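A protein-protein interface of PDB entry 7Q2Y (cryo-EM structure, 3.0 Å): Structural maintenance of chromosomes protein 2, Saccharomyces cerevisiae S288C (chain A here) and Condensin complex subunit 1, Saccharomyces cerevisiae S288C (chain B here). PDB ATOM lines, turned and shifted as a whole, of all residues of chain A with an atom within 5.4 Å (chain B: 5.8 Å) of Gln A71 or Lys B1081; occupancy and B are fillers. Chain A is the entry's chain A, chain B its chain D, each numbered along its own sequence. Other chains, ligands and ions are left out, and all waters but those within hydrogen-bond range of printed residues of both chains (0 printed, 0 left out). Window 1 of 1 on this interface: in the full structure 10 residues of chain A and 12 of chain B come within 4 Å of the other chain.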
ATOM      1  N   GLN A  63      35.352   7.879  14.226  1.00  0.00           N
ATOM      2  CA  GLN A  63      33.895   7.800  14.199  1.00  0.00           C
ATOM      3  C   GLN A  63      33.376   6.410  14.544  1.00  0.00           C
ATOM      4  O   GLN A  63      32.342   6.291  15.211  1.00  0.00           O
ATOM      5  CB  GLN A  63      33.372   8.224  12.825  1.00  0.00           C
ATOM      6  CG  GLN A  63      31.882   8.522  12.795  1.00  0.00           C
ATOM      7  CD  GLN A  63      31.413   9.013  11.440  1.00  0.00           C
ATOM      8  OE1 GLN A  63      30.521   8.425  10.829  1.00  0.00           O
ATOM      9  NE2 GLN A  63      32.015  10.096  10.962  1.00  0.00           N
ATOM     10  N   LYS A  68      27.325   3.019  16.798  1.00  0.00           N
ATOM     11  CA  LYS A  68      27.157   2.715  15.372  1.00  0.00           C
ATOM     12  C   LYS A  68      27.493   3.978  14.583  1.00  0.00           C
ATOM     13  O   LYS A  68      26.597   4.746  14.222  1.00  0.00           O
ATOM     14  CB  LYS A  68      25.749   2.217  15.074  1.00  0.00           C
ATOM     15  CG  LYS A  68      25.542   0.738  15.355  1.00  0.00           C
ATOM     16  CD  LYS A  68      24.066   0.375  15.339  1.00  0.00           C
ATOM     17  CE  LYS A  68      23.831  -1.008  15.924  1.00  0.00           C
ATOM     18  NZ  LYS A  68      22.430  -1.464  15.718  1.00  0.00           N
ATOM     19  N   ARG A  69      28.782   4.157  14.289  1.00  0.00           N
ATOM     20  CA  ARG A  69      29.313   5.332  13.580  1.00  0.00           C
ATOM     21  C   ARG A  69      28.710   6.579  14.228  1.00  0.00           C
ATOM     22  O   ARG A  69      28.652   6.652  15.463  1.00  0.00           O
ATOM     23  CB  ARG A  69      29.052   5.173  12.088  1.00  0.00           C
ATOM     24  CG  ARG A  69      29.767   3.990  11.458  1.00  0.00           C
ATOM     25  CD  ARG A  69      31.269   4.199  11.450  1.00  0.00           C
ATOM     26  NE  ARG A  69      31.657   5.376  10.683  1.00  0.00           N
ATOM     27  CZ  ARG A  69      31.867   5.379   9.374  1.00  0.00           C
ATOM     28  NH1 ARG A  69      31.745   4.276   8.653  1.00  0.00           N
ATOM     29  NH2 ARG A  69      32.211   6.515   8.775  1.00  0.00           N
ATOM     30  N   GLY A  70      28.255   7.561  13.460  1.00  0.00           N
ATOM     31  CA  GLY A  70      27.512   8.676  14.002  1.00  0.00           C
ATOM     32  C   GLY A  70      26.017   8.460  14.043  1.00  0.00           C
ATOM     33  O   GLY A  70      25.272   9.392  14.361  1.00  0.00           O
ATOM     34  N   GLN A  71      25.557   7.254  13.731  1.00  0.00           N
ATOM     35  CA  GLN A  71      24.148   6.936  13.604  1.00  0.00           C
ATOM     36  C   GLN A  71      23.665   6.186  14.845  1.00  0.00           C
ATOM     37  O   GLN A  71      24.372   6.084  15.853  1.00  0.00           O
ATOM     38  CB  GLN A  71      23.913   6.130  12.323  1.00  0.00           C
ATOM     39  CG  GLN A  71      24.039   6.942  11.039  1.00  0.00           C
ATOM     40  CD  GLN A  71      25.464   7.366  10.740  1.00  0.00           C
ATOM     41  OE1 GLN A  71      25.766   8.556  10.660  1.00  0.00           O
ATOM     42  NE2 GLN A  71      26.348   6.390  10.569  1.00  0.00           N
ATOM     43  N   ALA A  72      22.435   5.674  14.778  1.00  0.00           N
ATOM     44  CA  ALA A  72      21.770   4.864  15.797  1.00  0.00           C
ATOM     45  C   ALA A  72      21.436   5.644  17.061  1.00  0.00           C
ATOM     46  O   ALA A  72      21.086   5.027  18.074  1.00  0.00           O
ATOM     47  CB  ALA A  72      22.583   3.620  16.185  1.00  0.00           C
ATOM     48  N   GLY A  73      21.529   6.971  17.044  1.00  0.00           N
ATOM     49  CA  GLY A  73      21.142   7.763  18.193  1.00  0.00           C
ATOM     50  C   GLY A  73      22.305   8.171  19.072  1.00  0.00           C
ATOM     51  O   GLY A  73      22.350   9.302  19.566  1.00  0.00           O
ATOM     52  N   VAL A  74      23.255   7.261  19.276  1.00  0.00           N
ATOM     53  CA  VAL A  74      24.409   7.561  20.114  1.00  0.00           C
ATOM     54  C   VAL A  74      25.327   8.528  19.381  1.00  0.00           C
ATOM     55  O   VAL A  74      25.732   8.282  18.238  1.00  0.00           O
ATOM     56  CB  VAL A  74      25.147   6.271  20.498  1.00  0.00           C
ATOM     57  CG1 VAL A  74      26.309   6.582  21.430  1.00  0.00           C
ATOM     58  CG2 VAL A  74      24.187   5.287  21.148  1.00  0.00           C
ATOM     59  N   LEU B1043      19.943   3.119   9.502  1.00  0.00           N
ATOM     60  CA  LEU B1043      20.591   3.571  10.729  1.00  0.00           C
ATOM     61  C   LEU B1043      20.774   2.429  11.720  1.00  0.00           C
ATOM     62  O   LEU B1043      21.767   2.406  12.456  1.00  0.00           O
ATOM     63  CB  LEU B1043      19.793   4.709  11.369  1.00  0.00           C
ATOM     64  CG  LEU B1043      19.578   5.969  10.522  1.00  0.00           C
ATOM     65  CD1 LEU B1043      19.106   7.135  11.378  1.00  0.00           C
ATOM     66  CD2 LEU B1043      20.826   6.337   9.741  1.00  0.00           C
ATOM     67  N   THR B1076      21.039  11.979  -0.398  1.00  0.00           N
ATOM     68  CA  THR B1076      21.811  13.114   0.174  1.00  0.00           C
ATOM     69  C   THR B1076      22.023  12.970   1.678  1.00  0.00           C
ATOM     70  O   THR B1076      22.996  13.536   2.182  1.00  0.00           O
ATOM     71  CB  THR B1076      21.092  14.446  -0.022  1.00  0.00           C
ATOM     72  OG1 THR B1076      19.732  14.300   0.380  1.00  0.00           O
ATOM     73  CG2 THR B1076      21.170  14.982  -1.434  1.00  0.00           C
ATOM     74  N   GLU B1077      21.127  12.278   2.370  1.00  0.00           N
ATOM     75  CA  GLU B1077      21.229  12.195   3.844  1.00  0.00           C
ATOM     76  C   GLU B1077      21.779  10.833   4.214  1.00  0.00           C
ATOM     77  O   GLU B1077      22.702  10.784   5.020  1.00  0.00           O
ATOM     78  CB  GLU B1077      19.853  12.332   4.479  1.00  0.00           C
ATOM     79  CG  GLU B1077      19.605  13.701   5.083  1.00  0.00           C
ATOM     80  CD  GLU B1077      19.129  14.751   4.095  1.00  0.00           C
ATOM     81  OE1 GLU B1077      19.110  14.459   2.887  1.00  0.00           O
ATOM     82  OE2 GLU B1077      18.775  15.860   4.540  1.00  0.00           O
ATOM     83  N   LEU B1078      21.233   9.780   3.625  1.00  0.00           N
ATOM     84  CA  LEU B1078      21.649   8.429   3.979  1.00  0.00           C
ATOM     85  C   LEU B1078      22.811   7.925   3.133  1.00  0.00           C
ATOM     86  O   LEU B1078      23.758   7.343   3.670  1.00  0.00           O
ATOM     87  CB  LEU B1078      20.464   7.471   3.854  1.00  0.00           C
ATOM     88  CG  LEU B1078      19.414   7.600   4.955  1.00  0.00           C
ATOM     89  CD1 LEU B1078      18.086   7.061   4.475  1.00  0.00           C
ATOM     90  CD2 LEU B1078      19.870   6.876   6.209  1.00  0.00           C
ATOM     91  N   ALA B1079      22.754   8.132   1.816  1.00  0.00           N
ATOM     92  CA  ALA B1079      23.813   7.633   0.945  1.00  0.00           C
ATOM     93  C   ALA B1079      25.136   8.347   1.194  1.00  0.00           C
ATOM     94  O   ALA B1079      26.201   7.733   1.068  1.00  0.00           O
ATOM     95  CB  ALA B1079      23.399   7.776  -0.519  1.00  0.00           C
ATOM     96  N   SER B1080      25.091   9.626   1.559  1.00  0.00           N
ATOM     97  CA  SER B1080      26.289  10.434   1.733  1.00  0.00           C
ATOM     98  C   SER B1080      26.871  10.348   3.139  1.00  0.00           C
ATOM     99  O   SER B1080      27.833  11.061   3.440  1.00  0.00           O
ATOM    100  CB  SER B1080      25.992  11.895   1.385  1.00  0.00           C
ATOM    101  OG  SER B1080      25.411  12.573   2.486  1.00  0.00           O
ATOM    102  N   LYS B1081      26.305   9.505   4.006  1.00  0.00           N
ATOM    103  CA  LYS B1081      26.831   9.367   5.361  1.00  0.00           C
ATOM    104  C   LYS B1081      28.258   8.832   5.343  1.00  0.00           C
ATOM    105  O   LYS B1081      29.202   9.516   5.758  1.00  0.00           O
ATOM    106  CB  LYS B1081      25.923   8.451   6.185  1.00  0.00           C
ATOM    107  CG  LYS B1081      24.749   9.157   6.839  1.00  0.00           C
ATOM    108  CD  LYS B1081      25.216  10.152   7.887  1.00  0.00           C
ATOM    109  CE  LYS B1081      24.040  10.735   8.654  1.00  0.00           C
ATOM    110  NZ  LYS B1081      22.882  11.022   7.763  1.00  0.00           N
ATOM    111  N   ASP B1082      28.435   7.606   4.863  1.00  0.00           N
ATOM    112  CA  ASP B1082      29.734   6.964   4.790  1.00  0.00           C
ATOM    113  C   ASP B1082      30.324   7.146   3.392  1.00  0.00           C
ATOM    114  O   ASP B1082      29.792   7.886   2.559  1.00  0.00           O
ATOM    115  CB  ASP B1082      29.603   5.486   5.169  1.00  0.00           C
ATOM    116  CG  ASP B1082      30.891   4.909   5.722  1.00  0.00           C
ATOM    117  OD1 ASP B1082      31.899   5.645   5.778  1.00  0.00           O
ATOM    118  OD2 ASP B1082      30.896   3.719   6.102  1.00  0.00           O
ATOM    119  N   ASN B1083      31.437   6.463   3.127  1.00  0.00           N
ATOM    120  CA  ASN B1083      32.067   6.456   1.813  1.00  0.00           C
ATOM    121  C   ASN B1083      31.405   5.480   0.849  1.00  0.00           C
ATOM    122  O   ASN B1083      32.023   5.096  -0.156  1.00  0.00           O
ATOM    123  CB  ASN B1083      33.557   6.135   1.946  1.00  0.00           C
ATOM    124  CG  ASN B1083      34.281   7.095   2.870  1.00  0.00           C
ATOM    125  OD1 ASN B1083      34.389   8.287   2.585  1.00  0.00           O
ATOM    126  ND2 ASN B1083      34.781   6.578   3.987  1.00  0.00           N
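Among the printed residues, merely in contact across the chains: Gln A71 with Leu B1043 (3.5 Å) and Gln A71 with Lys B1081 (3.2 Å).
Of the printed residues of chain B, Arg A69 touches Asp B1082. Printed residues of chain B within 4 Å of Gln A71: Leu B1043 (3.5 Å) and Lys B1081 (3.2 Å). Of the printed residues of chain A, Leu B1043 touches Gln A71 (3.5 Å). Lys B1081 touches one residue of chain A. The nearest printed residue of chain B that does not touch Gln A71 is Asp B1082 (6.2 Å). The nearest residue of chain A that does not touch Lys B1081 is Arg A69 (5.2 Å). The nearest printed residue of chain A that does not touch Leu B1043 is Ala A72 (4.01 Å).
The guanidinium group (NE) of Arg A69 sits at hydrogen-bond distance from the side-chain amide oxygen (OE1) of Gln A63, at 3.3 Å. The backbone carbonyl oxygen (O) of Glu B1077 lies within hydrogen-bond range of the side-chain amino group (NZ) of Lys B1081, 2.8 Å away.
Of the 9 printed residues of chain B, 3 touch a printed residue of chain A. Hydrophobic or aromatic side chains of chain B within 4 Å of the printed part of chain A: Leu B1043. Of the 8 printed residues of chain A, 2 touch a printed residue of chain B. Printed residues of chain A that touch a printed residue of chain B: Arg A69 and Gln A71. Along chain A the printed residues that touch a printed residue of chain B span positions 69 to 71.
NH1 of Arg A69 lies within salt-bridge range of OD2 of Asp B1082, 2.7 Å away.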
